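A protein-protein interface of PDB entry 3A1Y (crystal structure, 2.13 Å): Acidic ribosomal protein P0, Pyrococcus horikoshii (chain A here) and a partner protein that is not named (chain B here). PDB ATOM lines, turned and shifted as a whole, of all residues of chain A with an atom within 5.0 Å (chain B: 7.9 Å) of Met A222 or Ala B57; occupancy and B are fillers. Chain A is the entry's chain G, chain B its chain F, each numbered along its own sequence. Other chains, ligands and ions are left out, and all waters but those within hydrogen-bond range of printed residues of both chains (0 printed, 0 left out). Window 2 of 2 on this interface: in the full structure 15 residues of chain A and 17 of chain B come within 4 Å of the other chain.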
ATOM      1  N   GLN A 218       6.887  15.566 -28.556  1.00  0.00           N
ATOM      2  CA  GLN A 218       6.619  17.008 -28.451  1.00  0.00           C
ATOM      3  C   GLN A 218       6.779  17.483 -27.008  1.00  0.00           C
ATOM      4  O   GLN A 218       7.294  18.569 -26.763  1.00  0.00           O
ATOM      5  CB  GLN A 218       5.201  17.330 -28.953  1.00  0.00           C
ATOM      6  CG  GLN A 218       4.994  17.075 -30.442  1.00  0.00           C
ATOM      7  CD  GLN A 218       3.589  17.411 -30.914  1.00  0.00           C
ATOM      8  OE1 GLN A 218       2.600  16.975 -30.327  1.00  0.00           O
ATOM      9  NE2 GLN A 218       3.497  18.197 -31.990  1.00  0.00           N
ATOM     10  N   LYS A 219       6.322  16.676 -26.053  1.00  0.00           N
ATOM     11  CA  LYS A 219       6.543  16.983 -24.626  1.00  0.00           C
ATOM     12  C   LYS A 219       8.028  17.067 -24.265  1.00  0.00           C
ATOM     13  O   LYS A 219       8.459  18.000 -23.597  1.00  0.00           O
ATOM     14  CB  LYS A 219       5.840  15.959 -23.725  1.00  0.00           C
ATOM     15  CG  LYS A 219       5.790  16.328 -22.240  1.00  0.00           C
ATOM     16  CD  LYS A 219       4.706  17.353 -21.920  1.00  0.00           C
ATOM     17  CE  LYS A 219       3.337  16.706 -21.702  1.00  0.00           C
ATOM     18  NZ  LYS A 219       3.193  16.262 -20.286  1.00  0.00           N
ATOM     19  N   ALA A 220       8.799  16.082 -24.702  1.00  0.00           N
ATOM     20  CA  ALA A 220      10.237  16.078 -24.466  1.00  0.00           C
ATOM     21  C   ALA A 220      10.918  17.278 -25.129  1.00  0.00           C
ATOM     22  O   ALA A 220      11.757  17.924 -24.514  1.00  0.00           O
ATOM     23  CB  ALA A 220      10.858  14.771 -24.951  1.00  0.00           C
ATOM     24  N   TYR A 221      10.527  17.604 -26.358  1.00  0.00           N
ATOM     25  CA  TYR A 221      11.045  18.820 -26.999  1.00  0.00           C
ATOM     26  C   TYR A 221      10.703  20.083 -26.181  1.00  0.00           C
ATOM     27  O   TYR A 221      11.556  20.944 -25.971  1.00  0.00           O
ATOM     28  CB  TYR A 221      10.531  18.967 -28.434  1.00  0.00           C
ATOM     29  CG  TYR A 221      10.963  20.268 -29.049  1.00  0.00           C
ATOM     30  CD1 TYR A 221      12.223  20.389 -29.641  1.00  0.00           C
ATOM     31  CD2 TYR A 221      10.126  21.389 -29.022  1.00  0.00           C
ATOM     32  CE1 TYR A 221      12.652  21.602 -30.180  1.00  0.00           C
ATOM     33  CE2 TYR A 221      10.533  22.610 -29.581  1.00  0.00           C
ATOM     34  CZ  TYR A 221      11.801  22.707 -30.151  1.00  0.00           C
ATOM     35  OH  TYR A 221      12.208  23.898 -30.717  1.00  0.00           O
ATOM     36  N   MET A 222       9.465  20.185 -25.721  1.00  0.00           N
ATOM     37  CA  MET A 222       9.060  21.343 -24.938  1.00  0.00           C
ATOM     38  C   MET A 222       9.792  21.439 -23.596  1.00  0.00           C
ATOM     39  O   MET A 222      10.152  22.530 -23.181  1.00  0.00           O
ATOM     40  CB  MET A 222       7.544  21.354 -24.718  1.00  0.00           C
ATOM     41  CG  MET A 222       6.704  21.880 -25.932  1.00  0.00           C
ATOM     42  SD  MET A 222       7.348  23.340 -26.798  1.00  0.00           S
ATOM     43  CE  MET A 222       7.398  24.584 -25.500  1.00  0.00           C
ATOM     44  N   HIS A 223       9.986  20.302 -22.928  1.00  0.00           N
ATOM     45  CA  HIS A 223      10.792  20.225 -21.698  1.00  0.00           C
ATOM     46  C   HIS A 223      12.189  20.802 -21.922  1.00  0.00           C
ATOM     47  O   HIS A 223      12.642  21.617 -21.142  1.00  0.00           O
ATOM     48  CB  HIS A 223      10.919  18.761 -21.212  1.00  0.00           C
ATOM     49  CG  HIS A 223       9.675  18.205 -20.590  1.00  0.00           C
ATOM     50  ND1 HIS A 223       8.624  18.999 -20.177  1.00  0.00           N
ATOM     51  CD2 HIS A 223       9.334  16.934 -20.264  1.00  0.00           C
ATOM     52  CE1 HIS A 223       7.681  18.236 -19.648  1.00  0.00           C
ATOM     53  NE2 HIS A 223       8.086  16.982 -19.693  1.00  0.00           N
ATOM     54  N   ALA A 224      12.867  20.374 -22.997  1.00  0.00           N
ATOM     55  CA  ALA A 224      14.193  20.909 -23.341  1.00  0.00           C
ATOM     56  C   ALA A 224      14.175  22.397 -23.668  1.00  0.00           C
ATOM     57  O   ALA A 224      15.036  23.138 -23.216  1.00  0.00           O
ATOM     58  CB  ALA A 224      14.792  20.139 -24.492  1.00  0.00           C
ATOM     59  N   PHE A 225      13.201  22.822 -24.474  1.00  0.00           N
ATOM     60  CA  PHE A 225      13.030  24.228 -24.773  1.00  0.00           C
ATOM     61  C   PHE A 225      12.819  25.051 -23.482  1.00  0.00           C
ATOM     62  O   PHE A 225      13.532  26.040 -23.251  1.00  0.00           O
ATOM     63  CB  PHE A 225      11.865  24.438 -25.776  1.00  0.00           C
ATOM     64  CG  PHE A 225      11.648  25.867 -26.145  1.00  0.00           C
ATOM     65  CD1 PHE A 225      12.442  26.481 -27.110  1.00  0.00           C
ATOM     66  CD2 PHE A 225      10.647  26.623 -25.520  1.00  0.00           C
ATOM     67  CE1 PHE A 225      12.229  27.842 -27.449  1.00  0.00           C
ATOM     68  CE2 PHE A 225      10.445  27.976 -25.849  1.00  0.00           C
ATOM     69  CZ  PHE A 225      11.236  28.578 -26.817  1.00  0.00           C
ATOM     70  N   ASN A 226      11.850  24.641 -22.650  1.00  0.00           N
ATOM     71  CA  ASN A 226      11.526  25.365 -21.395  1.00  0.00           C
ATOM     72  C   ASN A 226      12.690  25.420 -20.423  1.00  0.00           C
ATOM     73  O   ASN A 226      12.944  26.449 -19.800  1.00  0.00           O
ATOM     74  CB  ASN A 226      10.312  24.747 -20.694  1.00  0.00           C
ATOM     75  CG  ASN A 226       9.023  24.942 -21.477  1.00  0.00           C
ATOM     76  OD1 ASN A 226       8.903  25.887 -22.263  1.00  0.00           O
ATOM     77  ND2 ASN A 226       8.059  24.038 -21.278  1.00  0.00           N
ATOM     78  N   LEU A 227      13.395  24.307 -20.286  1.00  0.00           N
ATOM     79  CA  LEU A 227      14.557  24.279 -19.402  1.00  0.00           C
ATOM     80  C   LEU A 227      15.629  25.250 -19.896  1.00  0.00           C
ATOM     81  O   LEU A 227      16.119  26.081 -19.129  1.00  0.00           O
ATOM     82  CB  LEU A 227      15.129  22.857 -19.295  1.00  0.00           C
ATOM     83  CG  LEU A 227      16.433  22.687 -18.489  1.00  0.00           C
ATOM     84  CD1 LEU A 227      16.281  23.060 -17.002  1.00  0.00           C
ATOM     85  CD2 LEU A 227      16.954  21.269 -18.583  1.00  0.00           C
ATOM     86  N   TYR B   5      14.167  11.225 -25.292  1.00  0.00           N
ATOM     87  CA  TYR B   5      15.348  12.093 -25.258  1.00  0.00           C
ATOM     88  C   TYR B   5      16.510  11.525 -26.048  1.00  0.00           C
ATOM     89  O   TYR B   5      17.255  12.270 -26.671  1.00  0.00           O
ATOM     90  CB  TYR B   5      15.808  12.389 -23.816  1.00  0.00           C
ATOM     91  CG  TYR B   5      14.834  13.260 -23.059  1.00  0.00           C
ATOM     92  CD1 TYR B   5      14.474  14.514 -23.548  1.00  0.00           C
ATOM     93  CD2 TYR B   5      14.266  12.825 -21.850  1.00  0.00           C
ATOM     94  CE1 TYR B   5      13.563  15.334 -22.845  1.00  0.00           C
ATOM     95  CE2 TYR B   5      13.363  13.636 -21.152  1.00  0.00           C
ATOM     96  CZ  TYR B   5      13.013  14.881 -21.663  1.00  0.00           C
ATOM     97  OH  TYR B   5      12.124  15.691 -20.967  1.00  0.00           O
ATOM     98  N   LEU B   8      15.611  12.331 -29.689  1.00  0.00           N
ATOM     99  CA  LEU B   8      15.770  13.757 -29.951  1.00  0.00           C
ATOM    100  C   LEU B   8      17.247  14.138 -30.020  1.00  0.00           C
ATOM    101  O   LEU B   8      17.641  14.937 -30.850  1.00  0.00           O
ATOM    102  CB  LEU B   8      15.081  14.544 -28.849  1.00  0.00           C
ATOM    103  CG  LEU B   8      13.794  15.235 -29.289  1.00  0.00           C
ATOM    104  CD1 LEU B   8      13.148  14.638 -30.546  1.00  0.00           C
ATOM    105  CD2 LEU B   8      12.856  15.364 -28.125  1.00  0.00           C
ATOM    106  N   ILE B  50      10.168  14.202 -37.976  1.00  0.00           N
ATOM    107  CA  ILE B  50      10.427  14.731 -36.634  1.00  0.00           C
ATOM    108  C   ILE B  50      10.454  16.256 -36.598  1.00  0.00           C
ATOM    109  O   ILE B  50       9.929  16.867 -35.671  1.00  0.00           O
ATOM    110  CB  ILE B  50      11.672  14.066 -35.974  1.00  0.00           C
ATOM    111  CG1 ILE B  50      11.326  12.615 -35.608  1.00  0.00           C
ATOM    112  CG2 ILE B  50      12.107  14.802 -34.711  1.00  0.00           C
ATOM    113  CD1 ILE B  50      12.470  11.654 -35.722  1.00  0.00           C
ATOM    114  N   ASP B  51      11.023  16.863 -37.634  1.00  0.00           N
ATOM    115  CA  ASP B  51      11.101  18.320 -37.727  1.00  0.00           C
ATOM    116  C   ASP B  51       9.731  18.979 -37.812  1.00  0.00           C
ATOM    117  O   ASP B  51       9.522  20.023 -37.220  1.00  0.00           O
ATOM    118  CB  ASP B  51      12.020  18.700 -38.879  1.00  0.00           C
ATOM    119  CG  ASP B  51      13.288  17.871 -38.860  1.00  0.00           C
ATOM    120  OD1 ASP B  51      13.239  16.668 -39.279  1.00  0.00           O
ATOM    121  OD2 ASP B  51      14.300  18.399 -38.345  1.00  0.00           O
ATOM    122  N   GLU B  52       8.792  18.339 -38.500  1.00  0.00           N
ATOM    123  CA  GLU B  52       7.402  18.795 -38.519  1.00  0.00           C
ATOM    124  C   GLU B  52       6.697  18.632 -37.184  1.00  0.00           C
ATOM    125  O   GLU B  52       5.998  19.531 -36.729  1.00  0.00           O
ATOM    126  CB  GLU B  52       6.617  18.070 -39.611  1.00  0.00           C
ATOM    127  CG  GLU B  52       6.825  18.657 -40.960  1.00  0.00           C
ATOM    128  CD  GLU B  52       6.151  20.006 -41.130  1.00  0.00           C
ATOM    129  OE1 GLU B  52       5.006  20.186 -40.654  1.00  0.00           O
ATOM    130  OE2 GLU B  52       6.766  20.880 -41.766  1.00  0.00           O
ATOM    131  N   VAL B  53       6.873  17.469 -36.570  1.00  0.00           N
ATOM    132  CA  VAL B  53       6.374  17.204 -35.228  1.00  0.00           C
ATOM    133  C   VAL B  53       6.822  18.291 -34.234  1.00  0.00           C
ATOM    134  O   VAL B  53       6.005  18.803 -33.459  1.00  0.00           O
ATOM    135  CB  VAL B  53       6.813  15.790 -34.750  1.00  0.00           C
ATOM    136  CG1 VAL B  53       6.582  15.606 -33.258  1.00  0.00           C
ATOM    137  CG2 VAL B  53       6.066  14.726 -35.529  1.00  0.00           C
ATOM    138  N   ILE B  54       8.118  18.622 -34.272  1.00  0.00           N
ATOM    139  CA  ILE B  54       8.745  19.641 -33.411  1.00  0.00           C
ATOM    140  C   ILE B  54       8.207  21.059 -33.657  1.00  0.00           C
ATOM    141  O   ILE B  54       7.957  21.801 -32.711  1.00  0.00           O
ATOM    142  CB  ILE B  54      10.306  19.622 -33.568  1.00  0.00           C
ATOM    143  CG1 ILE B  54      10.928  18.478 -32.742  1.00  0.00           C
ATOM    144  CG2 ILE B  54      10.942  20.981 -33.200  1.00  0.00           C
ATOM    145  CD1 ILE B  54      12.424  18.296 -32.971  1.00  0.00           C
ATOM    146  N   GLU B  55       8.033  21.430 -34.928  1.00  0.00           N
ATOM    147  CA  GLU B  55       7.538  22.769 -35.274  1.00  0.00           C
ATOM    148  C   GLU B  55       6.083  22.959 -34.810  1.00  0.00           C
ATOM    149  O   GLU B  55       5.666  24.082 -34.510  1.00  0.00           O
ATOM    150  CB  GLU B  55       7.732  23.081 -36.776  1.00  0.00           C
ATOM    151  CG  GLU B  55       6.545  22.750 -37.688  1.00  0.00           C
ATOM    152  CD  GLU B  55       6.639  23.398 -39.079  1.00  0.00           C
ATOM    153  OE1 GLU B  55       7.647  23.182 -39.791  1.00  0.00           O
ATOM    154  OE2 GLU B  55       5.686  24.107 -39.470  1.00  0.00           O
ATOM    155  N   LYS B  56       5.338  21.852 -34.718  1.00  0.00           N
ATOM    156  CA  LYS B  56       3.973  21.856 -34.172  1.00  0.00           C
ATOM    157  C   LYS B  56       3.914  21.902 -32.624  1.00  0.00           C
ATOM    158  O   LYS B  56       2.835  21.999 -32.034  1.00  0.00           O
ATOM    159  CB  LYS B  56       3.165  20.704 -34.775  1.00  0.00           C
ATOM    160  CG  LYS B  56       2.703  21.018 -36.205  1.00  0.00           C
ATOM    161  CD  LYS B  56       2.716  19.796 -37.112  1.00  0.00           C
ATOM    162  CE  LYS B  56       2.205  20.142 -38.517  1.00  0.00           C
ATOM    163  NZ  LYS B  56       2.291  18.978 -39.438  1.00  0.00           N
ATOM    164  N   ALA B  57       5.091  21.799 -31.997  1.00  0.00           N
ATOM    165  CA  ALA B  57       5.409  22.366 -30.657  1.00  0.00           C
ATOM    166  C   ALA B  57       4.360  22.307 -29.535  1.00  0.00           C
ATOM    167  O   ALA B  57       4.202  23.275 -28.775  1.00  0.00           O
ATOM    168  CB  ALA B  57       5.924  23.814 -30.816  1.00  0.00           C
ATOM    169  N   ALA B  58       3.685  21.163 -29.413  1.00  0.00           N
ATOM    170  CA  ALA B  58       2.638  20.963 -28.400  1.00  0.00           C
ATOM    171  C   ALA B  58       2.490  19.487 -28.033  1.00  0.00           C
ATOM    172  O   ALA B  58       1.673  18.756 -28.618  1.00  0.00           O
ATOM    173  CB  ALA B  58       1.292  21.541 -28.889  1.00  0.00           C
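The backbone carbonyl oxygen (O) of Val B53 sits at hydrogen-bond distance from the side-chain amide nitrogen (NE2) of Gln A218.
The side-chain amide oxygen (OE1) of Gln A218 sits close to the backbone carbonyl oxygen (O) of Ala B58.
SD of Met A222 lies close to O of Ala B57, at 3.7 Å.
Among the printed residues, merely in contact across the chains: Gln A218 with Lys B56, Gln A218 with Ala B57, Ala A220 with Tyr B5, Ala A220 with Leu B8, Tyr A221 with Leu B8, Tyr A221 with Ile B54 and His A223 with Tyr B5.
Met A222 touches just one residue of chain B: Ala B57 (3.7 Å).
Of chain A, only Gln A218 (3.9 Å) and Met A222 (3.7 Å) come within 4 Å of Ala B57.
Printed residues of chain B within 4 Å of Gln A218: Val B53, Lys B56, Ala B57 and Ala B58.
Of the printed residues of chain A, Leu B8 touches Ala A220 and Tyr A221.
Printed residues of chain B within 4 Å of His A223: Tyr B5 (3.1 Å).
Printed residues of chain A within 4 Å of Ile B54: Tyr A221 (3.5 Å).
Of the printed residues of chain A, Val B53 touches Gln A218 (3.0 Å).
The nearest residue of chain B that does not touch Met A222 is Ala B58 (4.7 Å).
Printed residues of chain B that touch a printed residue of chain A: Tyr B5, Leu B8, Val B53, Ile B54, Lys B56, Ala B57 and Ala B58.
Hydrophobic or aromatic side chains of chain B that line the printed part of chain A: Tyr B5, Leu B8, Val B53 and Ile B54.
Of the 10 printed residues of chain A, 5 touch a printed residue of chain B.
Hydrophobic or aromatic side chains of chain A that line the printed part of chain B: Ala A220, Tyr A221, Met A222 and His A223.
Along chain A the printed residues that touch a printed residue of chain B span positions 218 to 223.
Among the printed residues, 10 pairs touch across the chains.
Among the printed residues, no Asp or Glu carboxylate lies within 4 Å of a Lys or Arg side-chain nitrogen of the other chain.
The side-chain carboxylate (OE1) of Glu B52 lies within salt-bridge range of the side-chain amino group (NZ) of Lys B56 (3.2 Å).
O of Met A222 sits close to ND2 of Asn A226 (3.2 Å).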
